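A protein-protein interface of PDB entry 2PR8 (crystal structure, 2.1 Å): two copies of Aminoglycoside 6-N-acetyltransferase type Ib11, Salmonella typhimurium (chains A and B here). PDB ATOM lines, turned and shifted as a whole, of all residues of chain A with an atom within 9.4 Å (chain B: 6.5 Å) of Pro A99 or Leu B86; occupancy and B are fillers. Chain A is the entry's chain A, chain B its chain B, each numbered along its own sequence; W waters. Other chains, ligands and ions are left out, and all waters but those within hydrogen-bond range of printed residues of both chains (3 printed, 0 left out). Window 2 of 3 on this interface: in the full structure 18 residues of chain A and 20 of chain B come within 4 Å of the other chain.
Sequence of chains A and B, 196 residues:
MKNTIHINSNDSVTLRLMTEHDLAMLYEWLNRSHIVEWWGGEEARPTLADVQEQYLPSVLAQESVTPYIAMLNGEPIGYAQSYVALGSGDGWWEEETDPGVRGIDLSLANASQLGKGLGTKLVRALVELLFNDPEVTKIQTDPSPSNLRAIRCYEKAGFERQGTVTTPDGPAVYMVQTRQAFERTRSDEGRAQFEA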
ATOM      1  N   SER A  64     -24.551   3.725  12.753  1.00  0.00           N
ATOM      2  CA  SER A  64     -23.206   3.591  12.213  1.00  0.00           C
ATOM      3  C   SER A  64     -22.347   4.805  12.645  1.00  0.00           C
ATOM      4  O   SER A  64     -21.603   5.393  11.850  1.00  0.00           O
ATOM      5  CB  SER A  64     -23.265   3.421  10.678  1.00  0.00           C
ATOM      6  OG  SER A  64     -24.192   2.382  10.323  1.00  0.00           O
ATOM      7  N   TYR A  83     -18.705   8.771  11.402  1.00  0.00           N
ATOM      8  CA  TYR A  83     -19.924   8.108  10.965  1.00  0.00           C
ATOM      9  C   TYR A  83     -19.682   7.644   9.543  1.00  0.00           C
ATOM     10  O   TYR A  83     -18.837   8.223   8.868  1.00  0.00           O
ATOM     11  CB  TYR A  83     -21.127   9.061  11.030  1.00  0.00           C
ATOM     12  CG  TYR A  83     -20.893  10.381  10.296  1.00  0.00           C
ATOM     13  CD1 TYR A  83     -21.268  10.511   8.951  1.00  0.00           C
ATOM     14  CD2 TYR A  83     -20.302  11.495  10.932  1.00  0.00           C
ATOM     15  CE1 TYR A  83     -21.038  11.643   8.247  1.00  0.00           C
ATOM     16  CE2 TYR A  83     -20.094  12.706  10.223  1.00  0.00           C
ATOM     17  CZ  TYR A  83     -20.485  12.739   8.873  1.00  0.00           C
ATOM     18  OH  TYR A  83     -20.297  13.835   8.083  1.00  0.00           O
ATOM     19  N   VAL A  84     -20.382   6.592   9.118  1.00  0.00           N
ATOM     20  CA  VAL A  84     -20.445   6.207   7.711  1.00  0.00           C
ATOM     21  C   VAL A  84     -21.365   7.214   7.007  1.00  0.00           C
ATOM     22  O   VAL A  84     -22.516   7.370   7.416  1.00  0.00           O
ATOM     23  CB  VAL A  84     -20.989   4.764   7.562  1.00  0.00           C
ATOM     24  CG1 VAL A  84     -20.989   4.345   6.066  1.00  0.00           C
ATOM     25  CG2 VAL A  84     -20.112   3.776   8.380  1.00  0.00           C
ATOM     26  N   ALA A  85     -20.862   7.968   6.020  1.00  0.00           N
ATOM     27  CA  ALA A  85     -21.722   8.978   5.339  1.00  0.00           C
ATOM     28  C   ALA A  85     -22.930   8.315   4.664  1.00  0.00           C
ATOM     29  O   ALA A  85     -24.091   8.775   4.741  1.00  0.00           O
ATOM     30  CB  ALA A  85     -20.905   9.736   4.274  1.00  0.00           C
ATOM     31  N   LEU A  86     -22.606   7.281   3.899  1.00  0.00           N
ATOM     32  CA  LEU A  86     -23.600   6.616   3.051  1.00  0.00           C
ATOM     33  C   LEU A  86     -24.642   5.969   3.936  1.00  0.00           C
ATOM     34  O   LEU A  86     -24.287   5.240   4.894  1.00  0.00           O
ATOM     35  CB  LEU A  86     -22.880   5.557   2.162  1.00  0.00           C
ATOM     36  CG  LEU A  86     -23.822   4.749   1.303  1.00  0.00           C
ATOM     37  CD1 LEU A  86     -24.464   5.631   0.288  1.00  0.00           C
ATOM     38  CD2 LEU A  86     -23.095   3.607   0.636  1.00  0.00           C
ATOM     39  N   GLY A  87     -25.910   6.259   3.634  1.00  0.00           N
ATOM     40  CA  GLY A  87     -27.060   5.725   4.381  1.00  0.00           C
ATOM     41  C   GLY A  87     -27.360   6.442   5.688  1.00  0.00           C
ATOM     42  O   GLY A  87     -28.069   5.927   6.552  1.00  0.00           O
ATOM     43  N   SER A  88     -26.803   7.629   5.874  1.00  0.00           N
ATOM     44  CA  SER A  88     -26.998   8.336   7.137  1.00  0.00           C
ATOM     45  C   SER A  88     -28.467   8.714   7.395  1.00  0.00           C
ATOM     46  O   SER A  88     -28.916   8.725   8.544  1.00  0.00           O
ATOM     47  CB  SER A  88     -26.150   9.609   7.187  1.00  0.00           C
ATOM     48  OG  SER A  88     -24.789   9.331   7.388  1.00  0.00           O
ATOM     49  N   GLU A  96     -24.161  10.416  -1.503  1.00  0.00           N
ATOM     50  CA  GLU A  96     -22.998   9.540  -1.319  1.00  0.00           C
ATOM     51  C   GLU A  96     -23.205   8.181  -2.035  1.00  0.00           C
ATOM     52  O   GLU A  96     -24.317   7.682  -2.101  1.00  0.00           O
ATOM     53  CB  GLU A  96     -22.708   9.322   0.164  1.00  0.00           C
ATOM     54  CG  GLU A  96     -21.383   8.567   0.449  1.00  0.00           C
ATOM     55  CD  GLU A  96     -20.211   9.145  -0.305  1.00  0.00           C
ATOM     56  OE1 GLU A  96     -19.755  10.265   0.043  1.00  0.00           O
ATOM     57  OE2 GLU A  96     -19.747   8.489  -1.264  1.00  0.00           O
ATOM     58  N   THR A  97     -22.127   7.594  -2.555  1.00  0.00           N
ATOM     59  CA  THR A  97     -22.225   6.268  -3.188  1.00  0.00           C
ATOM     60  C   THR A  97     -21.262   5.258  -2.609  1.00  0.00           C
ATOM     61  O   THR A  97     -21.463   4.064  -2.761  1.00  0.00           O
ATOM     62  CB  THR A  97     -22.013   6.355  -4.731  1.00  0.00           C
ATOM     63  OG1 THR A  97     -20.720   6.900  -5.003  1.00  0.00           O
ATOM     64  CG2 THR A  97     -23.069   7.271  -5.348  1.00  0.00           C
ATOM     65  N   ASP A  98     -20.232   5.735  -1.919  1.00  0.00           N
ATOM     66  CA  ASP A  98     -19.131   4.874  -1.511  1.00  0.00           C
ATOM     67  C   ASP A  98     -19.255   4.575  -0.027  1.00  0.00           C
ATOM     68  O   ASP A  98     -19.259   5.495   0.786  1.00  0.00           O
ATOM     69  CB  ASP A  98     -17.786   5.544  -1.819  1.00  0.00           C
ATOM     70  CG  ASP A  98     -16.591   4.752  -1.332  1.00  0.00           C
ATOM     71  OD1 ASP A  98     -16.728   3.585  -0.878  1.00  0.00           O
ATOM     72  OD2 ASP A  98     -15.482   5.311  -1.387  1.00  0.00           O
ATOM     73  N   PRO A  99     -19.350   3.265   0.323  1.00  0.00           N
ATOM     74  CA  PRO A  99     -19.428   2.791   1.708  1.00  0.00           C
ATOM     75  C   PRO A  99     -18.193   3.129   2.555  1.00  0.00           C
ATOM     76  O   PRO A  99     -18.298   3.125   3.770  1.00  0.00           O
ATOM     77  CB  PRO A  99     -19.522   1.244   1.574  1.00  0.00           C
ATOM     78  CG  PRO A  99     -19.876   0.963   0.161  1.00  0.00           C
ATOM     79  CD  PRO A  99     -19.438   2.174  -0.674  1.00  0.00           C
ATOM     80  N   GLY A 100     -17.036   3.327   1.918  1.00  0.00           N
ATOM     81  CA  GLY A 100     -15.790   3.615   2.621  1.00  0.00           C
ATOM     82  C   GLY A 100     -15.620   5.073   3.078  1.00  0.00           C
ATOM     83  O   GLY A 100     -14.630   5.392   3.664  1.00  0.00           O
ATOM     84  N   VAL A 101     -16.560   5.960   2.773  1.00  0.00           N
ATOM     85  CA  VAL A 101     -16.436   7.363   3.207  1.00  0.00           C
ATOM     86  C   VAL A 101     -16.868   7.460   4.676  1.00  0.00           C
ATOM     87  O   VAL A 101     -17.970   6.978   5.064  1.00  0.00           O
ATOM     88  CB  VAL A 101     -17.267   8.302   2.367  1.00  0.00           C
ATOM     89  CG1 VAL A 101     -17.228   9.816   2.975  1.00  0.00           C
ATOM     90  CG2 VAL A 101     -16.798   8.259   0.896  1.00  0.00           C
ATOM     91  N   ARG A 102     -15.952   7.973   5.496  1.00  0.00           N
ATOM     92  CA  ARG A 102     -16.260   8.330   6.893  1.00  0.00           C
ATOM     93  C   ARG A 102     -16.269   9.825   7.067  1.00  0.00           C
ATOM     94  O   ARG A 102     -15.330  10.520   6.624  1.00  0.00           O
ATOM     95  CB  ARG A 102     -15.208   7.756   7.883  1.00  0.00           C
ATOM     96  CG  ARG A 102     -15.102   6.200   7.933  1.00  0.00           C
ATOM     97  CD  ARG A 102     -16.370   5.517   8.348  1.00  0.00           C
ATOM     98  NE  ARG A 102     -16.286   4.048   8.143  1.00  0.00           N
ATOM     99  CZ  ARG A 102     -16.584   3.415   7.017  1.00  0.00           C
ATOM    100  NH1 ARG A 102     -17.116   4.061   5.990  1.00  0.00           N
ATOM    101  NH2 ARG A 102     -16.451   2.103   6.947  1.00  0.00           N
ATOM    102  N   GLY A 103     -17.298  10.330   7.733  1.00  0.00           N
ATOM    103  CA  GLY A 103     -17.327  11.728   8.123  1.00  0.00           C
ATOM    104  C   GLY A 103     -16.880  11.835   9.570  1.00  0.00           C
ATOM    105  O   GLY A 103     -16.991  10.853  10.324  1.00  0.00           O
ATOM    106  N   ASP A 133      -8.574   1.463   9.615  1.00  0.00           N
ATOM    107  CA  ASP A 133      -9.598   0.523   9.135  1.00  0.00           C
ATOM    108  C   ASP A 133      -9.476   0.461   7.599  1.00  0.00           C
ATOM    109  O   ASP A 133      -9.668   1.474   6.913  1.00  0.00           O
ATOM    110  CB  ASP A 133     -10.980   0.997   9.666  1.00  0.00           C
ATOM    111  CG  ASP A 133     -12.170   0.218   9.101  1.00  0.00           C
ATOM    112  OD1 ASP A 133     -12.021  -0.521   8.116  1.00  0.00           O
ATOM    113  OD2 ASP A 133     -13.295   0.379   9.652  1.00  0.00           O
ATOM    114  N   PRO A 134      -9.079  -0.718   7.049  1.00  0.00           N
ATOM    115  CA  PRO A 134      -8.854  -0.822   5.600  1.00  0.00           C
ATOM    116  C   PRO A 134     -10.082  -0.556   4.735  1.00  0.00           C
ATOM    117  O   PRO A 134      -9.933  -0.331   3.553  1.00  0.00           O
ATOM    118  CB  PRO A 134      -8.338  -2.268   5.401  1.00  0.00           C
ATOM    119  CG  PRO A 134      -8.706  -2.996   6.627  1.00  0.00           C
ATOM    120  CD  PRO A 134      -8.742  -1.977   7.744  1.00  0.00           C
ATOM    121  N   GLU A 135     -11.271  -0.571   5.321  1.00  0.00           N
ATOM    122  CA  GLU A 135     -12.504  -0.310   4.558  1.00  0.00           C
ATOM    123  C   GLU A 135     -12.690   1.188   4.311  1.00  0.00           C
ATOM    124  O   GLU A 135     -13.543   1.590   3.538  1.00  0.00           O
ATOM    125  CB  GLU A 135     -13.733  -0.827   5.300  1.00  0.00           C
ATOM    126  CG  GLU A 135     -13.928  -2.362   5.359  1.00  0.00           C
ATOM    127  CD  GLU A 135     -13.607  -3.076   4.064  1.00  0.00           C
ATOM    128  OE1 GLU A 135     -14.172  -2.708   2.987  1.00  0.00           O
ATOM    129  OE2 GLU A 135     -12.790  -4.017   4.129  1.00  0.00           O
ATOM    130  N   VAL A 136     -11.901   2.014   4.982  1.00  0.00           N
ATOM    131  CA  VAL A 136     -12.088   3.463   4.876  1.00  0.00           C
ATOM    132  C   VAL A 136     -11.327   4.006   3.660  1.00  0.00           C
ATOM    133  O   VAL A 136     -10.099   3.840   3.566  1.00  0.00           O
ATOM    134  CB  VAL A 136     -11.654   4.186   6.176  1.00  0.00           C
ATOM    135  CG1 VAL A 136     -11.818   5.737   6.011  1.00  0.00           C
ATOM    136  CG2 VAL A 136     -12.504   3.710   7.349  1.00  0.00           C
ATOM    137  N   THR A 137     -12.057   4.683   2.782  1.00  0.00           N
ATOM    138  CA  THR A 137     -11.512   5.201   1.528  1.00  0.00           C
ATOM    139  C   THR A 137     -11.247   6.725   1.527  1.00  0.00           C
ATOM    140  O   THR A 137     -10.374   7.225   0.787  1.00  0.00           O
ATOM    141  CB  THR A 137     -12.467   4.878   0.377  1.00  0.00           C
ATOM    142  OG1 THR A 137     -13.737   5.530   0.597  1.00  0.00           O
ATOM    143  CG2 THR A 137     -12.707   3.363   0.293  1.00  0.00           C
ATOM    144  N   LYS A 138     -12.007   7.464   2.331  1.00  0.00           N
ATOM    145  CA  LYS A 138     -11.973   8.928   2.272  1.00  0.00           C
ATOM    146  C   LYS A 138     -12.649   9.468   3.537  1.00  0.00           C
ATOM    147  O   LYS A 138     -13.570   8.849   4.054  1.00  0.00           O
ATOM    148  CB  LYS A 138     -12.748   9.381   1.008  1.00  0.00           C
ATOM    149  CG  LYS A 138     -12.855  10.887   0.787  1.00  0.00           C
ATOM    150  CD  LYS A 138     -13.268  11.209  -0.687  1.00  0.00           C
ATOM    151  CE  LYS A 138     -14.786  10.964  -0.827  1.00  0.00           C
ATOM    152  NZ  LYS A 138     -15.449  11.314  -2.146  1.00  0.00           N
ATOM    153  N   SER B  64     -20.168  -1.243  12.655  1.00  0.00           N
ATOM    154  CA  SER B  64     -21.589  -1.028  12.311  1.00  0.00           C
ATOM    155  C   SER B  64     -22.479  -2.218  12.735  1.00  0.00           C
ATOM    156  O   SER B  64     -23.410  -2.581  12.030  1.00  0.00           O
ATOM    157  CB  SER B  64     -21.738  -0.765  10.808  1.00  0.00           C
ATOM    158  OG  SER B  64     -20.831   0.242  10.389  1.00  0.00           O
ATOM    159  N   TYR B  83     -26.585  -5.851  11.802  1.00  0.00           N
ATOM    160  CA  TYR B  83     -25.429  -5.212  11.179  1.00  0.00           C
ATOM    161  C   TYR B  83     -25.870  -4.622   9.862  1.00  0.00           C
ATOM    162  O   TYR B  83     -26.846  -5.092   9.241  1.00  0.00           O
ATOM    163  CB  TYR B  83     -24.265  -6.195  10.977  1.00  0.00           C
ATOM    164  CG  TYR B  83     -24.622  -7.393  10.130  1.00  0.00           C
ATOM    165  CD1 TYR B  83     -24.487  -7.342   8.735  1.00  0.00           C
ATOM    166  CD2 TYR B  83     -25.091  -8.566  10.705  1.00  0.00           C
ATOM    167  CE1 TYR B  83     -24.851  -8.405   7.937  1.00  0.00           C
ATOM    168  CE2 TYR B  83     -25.439  -9.688   9.901  1.00  0.00           C
ATOM    169  CZ  TYR B  83     -25.302  -9.572   8.511  1.00  0.00           C
ATOM    170  OH  TYR B  83     -25.653 -10.604   7.657  1.00  0.00           O
ATOM    171  N   VAL B  84     -25.172  -3.580   9.453  1.00  0.00           N
ATOM    172  CA  VAL B  84     -25.334  -3.033   8.126  1.00  0.00           C
ATOM    173  C   VAL B  84     -24.602  -3.930   7.159  1.00  0.00           C
ATOM    174  O   VAL B  84     -23.395  -4.118   7.288  1.00  0.00           O
ATOM    175  CB  VAL B  84     -24.733  -1.611   8.078  1.00  0.00           C
ATOM    176  CG1 VAL B  84     -24.915  -0.996   6.641  1.00  0.00           C
ATOM    177  CG2 VAL B  84     -25.391  -0.732   9.205  1.00  0.00           C
ATOM    178  N   ALA B  85     -25.297  -4.477   6.163  1.00  0.00           N
ATOM    179  CA  ALA B  85     -24.643  -5.486   5.316  1.00  0.00           C
ATOM    180  C   ALA B  85     -23.623  -4.794   4.421  1.00  0.00           C
ATOM    181  O   ALA B  85     -22.480  -5.270   4.260  1.00  0.00           O
ATOM    182  CB  ALA B  85     -25.674  -6.204   4.466  1.00  0.00           C
ATOM    183  N   LEU B  86     -24.054  -3.687   3.825  1.00  0.00           N
ATOM    184  CA  LEU B  86     -23.209  -2.975   2.842  1.00  0.00           C
ATOM    185  C   LEU B  86     -21.965  -2.456   3.536  1.00  0.00           C
ATOM    186  O   LEU B  86     -22.067  -1.840   4.624  1.00  0.00           O
ATOM    187  CB  LEU B  86     -23.964  -1.773   2.247  1.00  0.00           C
ATOM    188  CG  LEU B  86     -23.186  -0.891   1.234  1.00  0.00           C
ATOM    189  CD1 LEU B  86     -22.843  -1.598  -0.020  1.00  0.00           C
ATOM    190  CD2 LEU B  86     -24.011   0.354   0.928  1.00  0.00           C
ATOM    191  N   GLY B  87     -20.806  -2.734   2.954  1.00  0.00           N
ATOM    192  CA  GLY B  87     -19.549  -2.207   3.475  1.00  0.00           C
ATOM    193  C   GLY B  87     -18.935  -2.980   4.645  1.00  0.00           C
ATOM    194  O   GLY B  87     -18.020  -2.500   5.272  1.00  0.00           O
ATOM    195  N   SER B  88     -19.403  -4.190   4.915  1.00  0.00           N
ATOM    196  CA  SER B  88     -18.905  -4.959   6.077  1.00  0.00           C
ATOM    197  C   SER B  88     -17.434  -5.347   6.012  1.00  0.00           C
ATOM    198  O   SER B  88     -16.754  -5.466   7.042  1.00  0.00           O
ATOM    199  CB  SER B  88     -19.719  -6.263   6.230  1.00  0.00           C
ATOM    200  OG  SER B  88     -21.085  -6.018   6.510  1.00  0.00           O
ATOM    201  N   GLY B  89     -16.919  -5.608   4.821  1.00  0.00           N
ATOM    202  CA  GLY B  89     -15.475  -6.005   4.779  1.00  0.00           C
ATOM    203  C   GLY B  89     -15.118  -7.384   5.380  1.00  0.00           C
ATOM    204  O   GLY B  89     -16.008  -8.151   5.751  1.00  0.00           O
ATOM    205  N   TRP B  92     -17.218  -9.806   3.559  1.00  0.00           N
ATOM    206  CA  TRP B  92     -18.631 -10.059   3.825  1.00  0.00           C
ATOM    207  C   TRP B  92     -19.533  -9.158   3.002  1.00  0.00           C
ATOM    208  O   TRP B  92     -19.326  -7.947   2.977  1.00  0.00           O
ATOM    209  CB  TRP B  92     -18.899  -9.860   5.329  1.00  0.00           C
ATOM    210  CG  TRP B  92     -18.408 -11.004   6.141  1.00  0.00           C
ATOM    211  CD1 TRP B  92     -17.217 -11.105   6.793  1.00  0.00           C
ATOM    212  CD2 TRP B  92     -19.090 -12.244   6.355  1.00  0.00           C
ATOM    213  NE1 TRP B  92     -17.118 -12.336   7.423  1.00  0.00           N
ATOM    214  CE2 TRP B  92     -18.255 -13.053   7.166  1.00  0.00           C
ATOM    215  CE3 TRP B  92     -20.335 -12.737   5.966  1.00  0.00           C
ATOM    216  CZ2 TRP B  92     -18.635 -14.344   7.597  1.00  0.00           C
ATOM    217  CZ3 TRP B  92     -20.707 -14.032   6.389  1.00  0.00           C
ATOM    218  CH2 TRP B  92     -19.855 -14.810   7.184  1.00  0.00           C
ATOM    219  N   TRP B  93     -20.549  -9.742   2.352  1.00  0.00           N
ATOM    220  CA  TRP B  93     -21.598  -8.981   1.623  1.00  0.00           C
ATOM    221  C   TRP B  93     -21.037  -8.036   0.545  1.00  0.00           C
ATOM    222  O   TRP B  93     -21.522  -6.942   0.356  1.00  0.00           O
ATOM    223  CB  TRP B  93     -22.609  -8.269   2.606  1.00  0.00           C
ATOM    224  CG  TRP B  93     -22.912  -9.203   3.737  1.00  0.00           C
ATOM    225  CD1 TRP B  93     -22.587  -9.041   5.044  1.00  0.00           C
ATOM    226  CD2 TRP B  93     -23.474 -10.507   3.610  1.00  0.00           C
ATOM    227  NE1 TRP B  93     -22.948 -10.166   5.758  1.00  0.00           N
ATOM    228  CE2 TRP B  93     -23.484 -11.086   4.895  1.00  0.00           C
ATOM    229  CE3 TRP B  93     -23.985 -11.244   2.524  1.00  0.00           C
ATOM    230  CZ2 TRP B  93     -24.000 -12.381   5.144  1.00  0.00           C
ATOM    231  CZ3 TRP B  93     -24.473 -12.550   2.761  1.00  0.00           C
ATOM    232  CH2 TRP B  93     -24.461 -13.097   4.077  1.00  0.00           C
ATOM    233  N   GLU B  94     -20.007  -8.489  -0.164  1.00  0.00           N
ATOM    234  CA  GLU B  94     -19.348  -7.646  -1.180  1.00  0.00           C
ATOM    235  C   GLU B  94     -20.229  -7.235  -2.377  1.00  0.00           C
ATOM    236  O   GLU B  94     -19.890  -6.298  -3.119  1.00  0.00           O
ATOM    237  CB  GLU B  94     -18.056  -8.306  -1.652  1.00  0.00           C
ATOM    238  CG  GLU B  94     -17.061  -8.469  -0.495  1.00  0.00           C
ATOM    239  CD  GLU B  94     -15.663  -8.081  -0.870  1.00  0.00           C
ATOM    240  OE1 GLU B  94     -15.451  -6.859  -1.143  1.00  0.00           O
ATOM    241  OE2 GLU B  94     -14.775  -8.966  -0.856  1.00  0.00           O
ATOM    242  N   GLU B  95     -21.340  -7.938  -2.574  1.00  0.00           N
ATOM    243  CA  GLU B  95     -22.203  -7.688  -3.728  1.00  0.00           C
ATOM    244  C   GLU B  95     -23.335  -6.756  -3.333  1.00  0.00           C
ATOM    245  O   GLU B  95     -24.143  -6.399  -4.176  1.00  0.00           O
ATOM    246  CB  GLU B  95     -22.871  -8.975  -4.213  1.00  0.00           C
ATOM    247  CG  GLU B  95     -21.983 -10.174  -4.397  1.00  0.00           C
ATOM    248  CD  GLU B  95     -21.495 -10.234  -5.783  1.00  0.00           C
ATOM    249  OE1 GLU B  95     -20.998  -9.165  -6.233  1.00  0.00           O
ATOM    250  OE2 GLU B  95     -21.633 -11.321  -6.415  1.00  0.00           O
ATOM    251  N   GLU B  96     -23.437  -6.422  -2.046  1.00  0.00           N
ATOM    252  CA  GLU B  96     -24.516  -5.575  -1.598  1.00  0.00           C
ATOM    253  C   GLU B  96     -24.329  -4.169  -2.213  1.00  0.00           C
ATOM    254  O   GLU B  96     -23.207  -3.743  -2.408  1.00  0.00           O
ATOM    255  CB  GLU B  96     -24.543  -5.485  -0.065  1.00  0.00           C
ATOM    256  CG  GLU B  96     -25.806  -4.758   0.493  1.00  0.00           C
ATOM    257  CD  GLU B  96     -27.125  -5.259  -0.063  1.00  0.00           C
ATOM    258  OE1 GLU B  96     -27.562  -6.409   0.270  1.00  0.00           O
ATOM    259  OE2 GLU B  96     -27.781  -4.478  -0.794  1.00  0.00           O
ATOM    260  N   THR B  97     -25.431  -3.474  -2.503  1.00  0.00           N
ATOM    261  CA  THR B  97     -25.364  -2.081  -2.951  1.00  0.00           C
ATOM    262  C   THR B  97     -26.290  -1.151  -2.166  1.00  0.00           C
ATOM    263  O   THR B  97     -26.133   0.070  -2.245  1.00  0.00           O
ATOM    264  CB  THR B  97     -25.770  -1.964  -4.445  1.00  0.00           C
ATOM    265  OG1 THR B  97     -27.112  -2.438  -4.583  1.00  0.00           O
ATOM    266  CG2 THR B  97     -24.822  -2.789  -5.346  1.00  0.00           C
ATOM    267  N   ASP B  98     -27.241  -1.722  -1.411  1.00  0.00           N
ATOM    268  CA  ASP B  98     -28.243  -0.931  -0.670  1.00  0.00           C
ATOM    269  C   ASP B  98     -27.869  -0.725   0.815  1.00  0.00           C
ATOM    270  O   ASP B  98     -27.826  -1.707   1.592  1.00  0.00           O
ATOM    271  CB  ASP B  98     -29.595  -1.634  -0.802  1.00  0.00           C
ATOM    272  CG  ASP B  98     -30.728  -0.929  -0.113  1.00  0.00           C
ATOM    273  OD1 ASP B  98     -30.571   0.149   0.487  1.00  0.00           O
ATOM    274  OD2 ASP B  98     -31.822  -1.509  -0.159  1.00  0.00           O
ATOM    275  N   PRO B  99     -27.621   0.554   1.231  1.00  0.00           N
ATOM    276  CA  PRO B  99     -27.379   0.856   2.654  1.00  0.00           C
ATOM    277  C   PRO B  99     -28.457   0.527   3.648  1.00  0.00           C
ATOM    278  O   PRO B  99     -28.128   0.367   4.836  1.00  0.00           O
ATOM    279  CB  PRO B  99     -27.135   2.397   2.683  1.00  0.00           C
ATOM    280  CG  PRO B  99     -27.606   2.934   1.386  1.00  0.00           C
ATOM    281  CD  PRO B  99     -27.431   1.766   0.389  1.00  0.00           C
ATOM    282  N   GLY B 100     -29.701   0.410   3.178  1.00  0.00           N
ATOM    283  CA  GLY B 100     -30.860   0.102   4.010  1.00  0.00           C
ATOM    284  C   GLY B 100     -30.973  -1.373   4.433  1.00  0.00           C
ATOM    285  O   GLY B 100     -31.859  -1.754   5.192  1.00  0.00           O
ATOM    286  N   VAL B 101     -30.097  -2.211   3.912  1.00  0.00           N
ATOM    287  CA  VAL B 101     -30.106  -3.639   4.264  1.00  0.00           C
ATOM    288  C   VAL B 101     -29.417  -3.854   5.598  1.00  0.00           C
ATOM    289  O   VAL B 101     -28.279  -3.384   5.835  1.00  0.00           O
ATOM    290  CB  VAL B 101     -29.483  -4.506   3.190  1.00  0.00           C
ATOM    291  CG1 VAL B 101     -29.532  -6.040   3.622  1.00  0.00           C
ATOM    292  CG2 VAL B 101     -30.259  -4.321   1.891  1.00  0.00           C
HETATM  293  O   HOH W   1     -22.654   1.357   8.227  1.00  0.00           O
HETATM  294  O   HOH W   2     -17.053   0.018   4.974  1.00  0.00           O
HETATM  295  O   HOH W   3     -29.081   3.347   6.379  1.00  0.00           O
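OD1 of Asp A133 sits at hydrogen-bond distance from N of Glu A135 (2.9 Å).
The backbone NH of Val A84 lies within hydrogen-bond range of the backbone carbonyl oxygen of Ser A64, at 3.2 Å.
The backbone carbonyl oxygen (O) of Val B84 is in hydrogen-bond range of the side-chain hydroxyl (OG) of Ser B88 (3.1 Å).
NH1 of Arg A102 sits at hydrogen-bond distance from O of Pro A99 (2.7 Å).
The backbone carbonyl oxygen (O) of Ser B64 is in hydrogen-bond range of the backbone NH (N) of Val B84 (3.3 Å).
Among the printed residues, pairs that only touch across the chains: Leu A86 with Leu B86, Glu A135 with Gly B89, Ser A64 with Val B84, Gly A87 with Pro B99, Pro A99 with Leu B86, Pro A99 with Gly B87 and Ser A64 with Ser B64.
Hydrophobic or aromatic side chains of chain B that line the printed part of chain A: Val B84, Leu B86 and Pro B99.
Along chain B the printed residues that touch a printed residue of chain A span positions 64 to 99.
Hydrophobic or aromatic side chains of chain A within 4 Å of the printed part of chain B: Leu A86 and Pro A99.
Among the printed residues, 7 pairs touch across the chains.
Among the printed residues, no Asp or Glu carboxylate lies within 4 Å of a Lys or Arg side-chain nitrogen of the other chain.
Water W2 bridges O of Gly B87 and NH2 of Arg A102.
Water W3 bridges O of Gly A87 (2.8 Å) and O of Pro B99 (3.5 Å).
Water W1 lies within hydrogen-bond range of OG of Ser A64 (2.8 Å) and OG of Ser B64 (3.0 Å).
Pro A99 touches just these residues of chain B: Leu B86 (3.9 Å) and Gly B87 (3.9 Å).
Of chain A, only Leu A86 (3.4 Å) and Pro A99 (3.9 Å) come within 4 Å of Leu B86.
Of the printed residues of chain B, Ser A64 touches Ser B64 (3.99 Å) and Val B84 (3.5 Å).
Of the printed residues of chain A, Ser B64 touches Ser A64 (3.99 Å).
Of the printed residues of chain A, Gly B89 touches Glu A135 (3.4 Å).
Asp A133 touches none of the printed residues of chain B.
The nearest residue of chain B that does not touch Pro A99 is Glu B96 (6.3 Å).
The nearest residue of chain A that does not touch Leu B86 is Thr A97 (5.8 Å).
Ser B64 touches its own counterpart, Ser A64.
Ser A64 touches Val B84, but with the chains exchanged Val A84 does not touch Ser B64 (4.1 Å).
Leu B86 touches its own counterpart, Leu A86.
Pro A99 touches Leu B86, but with the chains exchanged Leu A86 does not touch Pro B99 (4.2 Å).
Positions printed for both chains: 64, 83, 84, 85, 86, 87, 88, 96, 97, 98, 99, 100 and 101.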
